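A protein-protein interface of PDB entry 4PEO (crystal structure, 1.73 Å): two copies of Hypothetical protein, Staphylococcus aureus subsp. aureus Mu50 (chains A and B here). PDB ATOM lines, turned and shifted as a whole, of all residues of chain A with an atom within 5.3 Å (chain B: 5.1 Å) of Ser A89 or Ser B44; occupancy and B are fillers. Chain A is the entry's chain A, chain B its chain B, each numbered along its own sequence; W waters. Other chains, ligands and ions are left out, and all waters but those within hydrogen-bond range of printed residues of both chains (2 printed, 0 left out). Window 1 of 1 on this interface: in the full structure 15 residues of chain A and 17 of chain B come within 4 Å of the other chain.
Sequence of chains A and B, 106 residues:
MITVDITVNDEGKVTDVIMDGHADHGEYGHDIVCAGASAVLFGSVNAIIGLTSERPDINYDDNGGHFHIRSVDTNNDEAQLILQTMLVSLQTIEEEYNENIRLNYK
ND2 of Asn B46 lies within hydrogen-bond range of OG1 of Thr A92 (3.0 Å).
The side-chain hydroxyl (OG) of Ser A89 is in hydrogen-bond range of the backbone carbonyl oxygen (O) of Thr A85. O of Val A88 lies within hydrogen-bond range of OG1 of Thr A92 (2.8 Å). OG of Ser B44 is in hydrogen-bond range of O of Val B40 (2.7 Å).
Of the 12 printed residues of chain B, 6 touch a printed residue of chain A. Printed residues of chain B that touch a printed residue of chain A: Ala B39, Gly B43, Ser B44, Asn B46, Ala B47 and Ile B82. Of the 11 printed residues of chain A, 5 touch a printed residue of chain B. Hydrophobic or aromatic side chains of chain A within 4 Å of the printed part of chain B: Val A88 and Ile A93. Along chain A the printed residues that touch a printed residue of chain B span positions 85 to 93.
Thr A85 touches Ala B47 (CG2 to CB, 3.6 Å). Thr A85 touches Ile B82. CG1 of Val A88 touches O of Gly B43, at 3.9 Å. Asn B46 touches Val A88 (CB to CG1, 3.7 Å). Ala B47 touches Val A88. Gly B43 touches Ser A89 (C to OG, 3.3 Å). OG of Ser A89 touches N of Ser B44, 3.8 Å away. Ala B39 touches Ile A93 (CB to CD1, 3.8 Å).
Positions printed for both chains: 40 and 86.
Water W2 lies within hydrogen-bond range of the side-chain hydroxyl (OG) of Ser A89 (2.5 Å), the backbone carbonyl oxygen (O) of Val B40 (3.2 Å) and the side-chain hydroxyl (OG) of Ser B44 (3.3 Å). Water W1 lies within hydrogen-bond range of O of Ala B39 (2.7 Å) and O of Ser A89 (2.9 Å).
Of the printed residues of chain A, Gly B43 touches Val A88 and Ser A89. Of the printed residues of chain A, Ser B44 touches Ser A89. Of the printed residues of chain A, Asn B46 touches Val A88 and Thr A92. The nearest printed residue of chain B that does not touch Ser A89 is Ala B39 (4.3 Å). The nearest printed residue of chain A that does not touch Ile B82 is Gln A84 (7.2 Å).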
ATOM      1  N   VAL A  40     -32.911  23.712  12.058  1.00  0.00           N
ATOM      2  CA  VAL A  40     -32.174  23.134  13.188  1.00  0.00           C
ATOM      3  C   VAL A  40     -32.912  21.892  13.697  1.00  0.00           C
ATOM      4  O   VAL A  40     -32.289  20.850  13.900  1.00  0.00           O
ATOM      5  CB  VAL A  40     -31.938  24.199  14.291  1.00  0.00           C
ATOM      6  CG1 VAL A  40     -31.430  23.558  15.577  1.00  0.00           C
ATOM      7  CG2 VAL A  40     -30.977  25.283  13.801  1.00  0.00           C
ATOM      8  N   GLN A  84     -28.516  18.063  22.548  1.00  0.00           N
ATOM      9  CA  GLN A  84     -27.891  19.187  23.211  1.00  0.00           C
ATOM     10  C   GLN A  84     -27.376  20.194  22.186  1.00  0.00           C
ATOM     11  O   GLN A  84     -27.496  21.346  22.393  1.00  0.00           O
ATOM     12  CB  GLN A  84     -26.772  18.746  24.157  1.00  0.00           C
ATOM     13  CG  GLN A  84     -27.236  17.842  25.267  1.00  0.00           C
ATOM     14  CD  GLN A  84     -27.825  18.594  26.430  1.00  0.00           C
ATOM     15  OE1 GLN A  84     -27.764  19.805  26.497  1.00  0.00           O
ATOM     16  NE2 GLN A  84     -28.411  17.869  27.361  1.00  0.00           N
ATOM     17  N   THR A  85     -26.813  19.714  21.088  1.00  0.00           N
ATOM     18  CA  THR A  85     -26.336  20.583  19.992  1.00  0.00           C
ATOM     19  C   THR A  85     -27.527  21.386  19.416  1.00  0.00           C
ATOM     20  O   THR A  85     -27.409  22.589  19.153  1.00  0.00           O
ATOM     21  CB  THR A  85     -25.612  19.731  18.928  1.00  0.00           C
ATOM     22  OG1 THR A  85     -24.423  19.183  19.525  1.00  0.00           O
ATOM     23  CG2 THR A  85     -25.256  20.544  17.661  1.00  0.00           C
ATOM     24  N   MET A  86     -28.667  20.698  19.222  1.00  0.00           N
ATOM     25  CA  MET A  86     -29.887  21.294  18.704  1.00  0.00           C
ATOM     26  C   MET A  86     -30.314  22.406  19.675  1.00  0.00           C
ATOM     27  O   MET A  86     -30.644  23.498  19.229  1.00  0.00           O
ATOM     28  CB  MET A  86     -30.977  20.204  18.583  1.00  0.00           C
ATOM     29  CG  MET A  86     -32.162  20.602  17.671  1.00  0.00           C
ATOM     30  SD  MET A  86     -33.558  19.415  17.893  1.00  0.00           S
ATOM     31  CE  MET A  86     -33.864  19.860  19.357  1.00  0.00           C
ATOM     32  N   LEU A  87     -30.242  22.151  20.988  1.00  0.00           N
ATOM     33  CA  LEU A  87     -30.635  23.149  22.005  1.00  0.00           C
ATOM     34  C   LEU A  87     -29.708  24.351  22.021  1.00  0.00           C
ATOM     35  O   LEU A  87     -30.190  25.491  22.036  1.00  0.00           O
ATOM     36  CB  LEU A  87     -30.769  22.505  23.389  1.00  0.00           C
ATOM     37  CG  LEU A  87     -31.853  21.418  23.495  1.00  0.00           C
ATOM     38  CD1 LEU A  87     -31.905  20.864  24.871  1.00  0.00           C
ATOM     39  CD2 LEU A  87     -33.219  21.920  23.043  1.00  0.00           C
ATOM     40  N   VAL A  88     -28.382  24.118  21.926  1.00  0.00           N
ATOM     41  CA  VAL A  88     -27.415  25.221  21.832  1.00  0.00           C
ATOM     42  C   VAL A  88     -27.720  26.070  20.576  1.00  0.00           C
ATOM     43  O   VAL A  88     -27.688  27.316  20.646  1.00  0.00           O
ATOM     44  CB  VAL A  88     -25.956  24.702  21.871  1.00  0.00           C
ATOM     45  CG1 VAL A  88     -24.951  25.801  21.489  1.00  0.00           C
ATOM     46  CG2 VAL A  88     -25.628  24.123  23.242  1.00  0.00           C
ATOM     47  N   SER A  89     -28.031  25.404  19.443  1.00  0.00           N
ATOM     48  CA  SER A  89     -28.353  26.100  18.191  1.00  0.00           C
ATOM     49  C   SER A  89     -29.637  26.939  18.307  1.00  0.00           C
ATOM     50  O   SER A  89     -29.683  28.055  17.790  1.00  0.00           O
ATOM     51  CB  SER A  89     -28.480  25.111  17.038  1.00  0.00           C
ATOM     52  OG  SER A  89     -27.275  24.401  16.793  1.00  0.00           O
ATOM     53  N   LEU A  90     -30.659  26.412  19.008  1.00  0.00           N
ATOM     54  CA  LEU A  90     -31.932  27.130  19.219  1.00  0.00           C
ATOM     55  C   LEU A  90     -31.718  28.311  20.166  1.00  0.00           C
ATOM     56  O   LEU A  90     -32.257  29.396  19.925  1.00  0.00           O
ATOM     57  CB  LEU A  90     -33.022  26.192  19.746  1.00  0.00           C
ATOM     58  CG  LEU A  90     -33.536  25.118  18.758  1.00  0.00           C
ATOM     59  CD1 LEU A  90     -34.513  24.162  19.454  1.00  0.00           C
ATOM     60  CD2 LEU A  90     -34.180  25.742  17.507  1.00  0.00           C
ATOM     61  N   GLN A  91     -30.882  28.114  21.216  1.00  0.00           N
ATOM     62  CA  GLN A  91     -30.511  29.179  22.164  1.00  0.00           C
ATOM     63  C   GLN A  91     -29.776  30.299  21.425  1.00  0.00           C
ATOM     64  O   GLN A  91     -29.973  31.473  21.752  1.00  0.00           O
ATOM     65  CB  GLN A  91     -29.613  28.629  23.284  1.00  0.00           C
ATOM     66  CG  GLN A  91     -30.351  27.779  24.316  1.00  0.00           C
ATOM     67  CD  GLN A  91     -29.456  27.119  25.342  1.00  0.00           C
ATOM     68  OE1 GLN A  91     -28.245  26.947  25.152  1.00  0.00           O
ATOM     69  NE2 GLN A  91     -30.053  26.701  26.448  1.00  0.00           N
ATOM     70  N   THR A  92     -28.936  29.938  20.414  1.00  0.00           N
ATOM     71  CA  THR A  92     -28.199  30.906  19.587  1.00  0.00           C
ATOM     72  C   THR A  92     -29.199  31.779  18.795  1.00  0.00           C
ATOM     73  O   THR A  92     -29.051  33.000  18.780  1.00  0.00           O
ATOM     74  CB  THR A  92     -27.159  30.207  18.697  1.00  0.00           C
ATOM     75  OG1 THR A  92     -26.284  29.435  19.521  1.00  0.00           O
ATOM     76  CG2 THR A  92     -26.322  31.201  17.876  1.00  0.00           C
ATOM     77  N   ILE A  93     -30.229  31.157  18.187  1.00  0.00           N
ATOM     78  CA  ILE A  93     -31.294  31.884  17.459  1.00  0.00           C
ATOM     79  C   ILE A  93     -32.052  32.806  18.434  1.00  0.00           C
ATOM     80  O   ILE A  93     -32.246  33.985  18.120  1.00  0.00           O
ATOM     81  CB  ILE A  93     -32.287  30.925  16.714  1.00  0.00           C
ATOM     82  CG1 ILE A  93     -31.568  30.047  15.686  1.00  0.00           C
ATOM     83  CG2 ILE A  93     -33.466  31.689  16.057  1.00  0.00           C
ATOM     84  CD1 ILE A  93     -32.363  28.775  15.283  1.00  0.00           C
ATOM     85  N   ALA B  39     -27.943  29.613  10.984  1.00  0.00           N
ATOM     86  CA  ALA B  39     -28.305  29.118  12.315  1.00  0.00           C
ATOM     87  C   ALA B  39     -27.655  27.763  12.588  1.00  0.00           C
ATOM     88  O   ALA B  39     -27.153  27.538  13.684  1.00  0.00           O
ATOM     89  CB  ALA B  39     -29.818  29.016  12.452  1.00  0.00           C
ATOM     90  N   VAL B  40     -27.652  26.875  11.583  1.00  0.00           N
ATOM     91  CA  VAL B  40     -27.056  25.539  11.696  1.00  0.00           C
ATOM     92  C   VAL B  40     -25.538  25.661  11.879  1.00  0.00           C
ATOM     93  O   VAL B  40     -24.968  25.021  12.763  1.00  0.00           O
ATOM     94  CB  VAL B  40     -27.435  24.647  10.479  1.00  0.00           C
ATOM     95  CG1 VAL B  40     -26.604  23.363  10.455  1.00  0.00           C
ATOM     96  CG2 VAL B  40     -28.919  24.311  10.489  1.00  0.00           C
ATOM     97  N   LEU B  41     -24.880  26.479  11.083  1.00  0.00           N
ATOM     98  CA  LEU B  41     -23.446  26.629  11.197  1.00  0.00           C
ATOM     99  C   LEU B  41     -23.005  27.284  12.503  1.00  0.00           C
ATOM    100  O   LEU B  41     -22.226  26.713  13.220  1.00  0.00           O
ATOM    101  CB  LEU B  41     -22.927  27.379   9.990  1.00  0.00           C
ATOM    102  CG  LEU B  41     -21.438  27.506   9.700  1.00  0.00           C
ATOM    103  CD1 LEU B  41     -20.559  27.941  10.827  1.00  0.00           C
ATOM    104  CD2 LEU B  41     -20.872  26.440   8.793  1.00  0.00           C
ATOM    105  N   PHE B  42     -23.521  28.477  12.797  1.00  0.00           N
ATOM    106  CA  PHE B  42     -23.129  29.167  14.030  1.00  0.00           C
ATOM    107  C   PHE B  42     -23.505  28.385  15.281  1.00  0.00           C
ATOM    108  O   PHE B  42     -22.700  28.301  16.205  1.00  0.00           O
ATOM    109  CB  PHE B  42     -23.650  30.614  14.070  1.00  0.00           C
ATOM    110  CG  PHE B  42     -23.237  31.465  12.884  1.00  0.00           C
ATOM    111  CD1 PHE B  42     -21.940  31.412  12.385  1.00  0.00           C
ATOM    112  CD2 PHE B  42     -24.134  32.348  12.297  1.00  0.00           C
ATOM    113  CE1 PHE B  42     -21.564  32.191  11.283  1.00  0.00           C
ATOM    114  CE2 PHE B  42     -23.759  33.127  11.199  1.00  0.00           C
ATOM    115  CZ  PHE B  42     -22.479  33.038  10.694  1.00  0.00           C
ATOM    116  N   GLY B  43     -24.683  27.756  15.263  1.00  0.00           N
ATOM    117  CA  GLY B  43     -25.155  26.946  16.378  1.00  0.00           C
ATOM    118  C   GLY B  43     -24.238  25.761  16.603  1.00  0.00           C
ATOM    119  O   GLY B  43     -23.908  25.452  17.750  1.00  0.00           O
ATOM    120  N   SER B  44     -23.777  25.120  15.509  1.00  0.00           N
ATOM    121  CA  SER B  44     -22.867  23.967  15.612  1.00  0.00           C
ATOM    122  C   SER B  44     -21.518  24.361  16.185  1.00  0.00           C
ATOM    123  O   SER B  44     -20.999  23.642  17.036  1.00  0.00           O
ATOM    124  CB  SER B  44     -22.708  23.261  14.275  1.00  0.00           C
ATOM    125  OG  SER B  44     -23.982  22.788  13.873  1.00  0.00           O
ATOM    126  N   VAL B  45     -20.975  25.535  15.776  1.00  0.00           N
ATOM    127  CA  VAL B  45     -19.704  26.036  16.329  1.00  0.00           C
ATOM    128  C   VAL B  45     -19.870  26.264  17.842  1.00  0.00           C
ATOM    129  O   VAL B  45     -19.036  25.798  18.624  1.00  0.00           O
ATOM    130  CB  VAL B  45     -19.228  27.315  15.581  1.00  0.00           C
ATOM    131  CG1 VAL B  45     -17.991  27.930  16.259  1.00  0.00           C
ATOM    132  CG2 VAL B  45     -18.927  26.999  14.121  1.00  0.00           C
ATOM    133  N   ASN B  46     -20.973  26.923  18.254  1.00  0.00           N
ATOM    134  CA  ASN B  46     -21.242  27.155  19.672  1.00  0.00           C
ATOM    135  C   ASN B  46     -21.370  25.840  20.447  1.00  0.00           C
ATOM    136  O   ASN B  46     -20.929  25.767  21.600  1.00  0.00           O
ATOM    137  CB  ASN B  46     -22.480  28.008  19.858  1.00  0.00           C
ATOM    138  CG  ASN B  46     -22.273  29.458  19.485  1.00  0.00           C
ATOM    139  OD1 ASN B  46     -21.150  29.937  19.304  1.00  0.00           O
ATOM    140  ND2 ASN B  46     -23.360  30.192  19.358  1.00  0.00           N
ATOM    141  N   ALA B  47     -21.944  24.800  19.807  1.00  0.00           N
ATOM    142  CA  ALA B  47     -22.102  23.481  20.439  1.00  0.00           C
ATOM    143  C   ALA B  47     -20.736  22.796  20.610  1.00  0.00           C
ATOM    144  O   ALA B  47     -20.481  22.192  21.660  1.00  0.00           O
ATOM    145  CB  ALA B  47     -23.041  22.599  19.615  1.00  0.00           C
ATOM    146  N   ILE B  48     -19.858  22.883  19.598  1.00  0.00           N
ATOM    147  CA  ILE B  48     -18.533  22.264  19.732  1.00  0.00           C
ATOM    148  C   ILE B  48     -17.806  22.891  20.941  1.00  0.00           C
ATOM    149  O   ILE B  48     -17.277  22.174  21.794  1.00  0.00           O
ATOM    150  CB  ILE B  48     -17.688  22.409  18.433  1.00  0.00           C
ATOM    151  CG1 ILE B  48     -18.272  21.572  17.282  1.00  0.00           C
ATOM    152  CG2 ILE B  48     -16.194  22.044  18.706  1.00  0.00           C
ATOM    153  CD1 ILE B  48     -17.676  21.932  15.855  1.00  0.00           C
ATOM    154  N   ILE B  82     -20.697  16.343  16.037  1.00  0.00           N
ATOM    155  CA  ILE B  82     -21.359  17.642  15.847  1.00  0.00           C
ATOM    156  C   ILE B  82     -21.163  18.138  14.410  1.00  0.00           C
ATOM    157  O   ILE B  82     -22.111  18.620  13.783  1.00  0.00           O
ATOM    158  CB  ILE B  82     -20.896  18.665  16.917  1.00  0.00           C
ATOM    159  CG1 ILE B  82     -21.364  18.195  18.328  1.00  0.00           C
ATOM    160  CG2 ILE B  82     -21.464  20.069  16.595  1.00  0.00           C
ATOM    161  CD1 ILE B  82     -20.760  19.014  19.499  1.00  0.00           C
ATOM    162  N   MET B  86     -24.018  18.791  11.686  1.00  0.00           N
ATOM    163  CA  MET B  86     -24.096  20.059  10.950  1.00  0.00           C
ATOM    164  C   MET B  86     -24.208  19.757   9.451  1.00  0.00           C
ATOM    165  O   MET B  86     -25.039  20.364   8.788  1.00  0.00           O
ATOM    166  CB  MET B  86     -22.811  20.861  11.218  1.00  0.00           C
ATOM    167  CG  MET B  86     -22.919  22.343  10.800  1.00  0.00           C
ATOM    168  SD  MET B  86     -21.248  23.159  10.862  1.00  0.00           S
ATOM    169  CE  MET B  86     -20.613  22.401   9.586  1.00  0.00           C
HETATM  170  O   HOH W   1     -27.887  29.078  15.827  1.00  0.00           O
HETATM  171  O   HOH W   2     -27.127  23.472  14.512  1.00  0.00           O
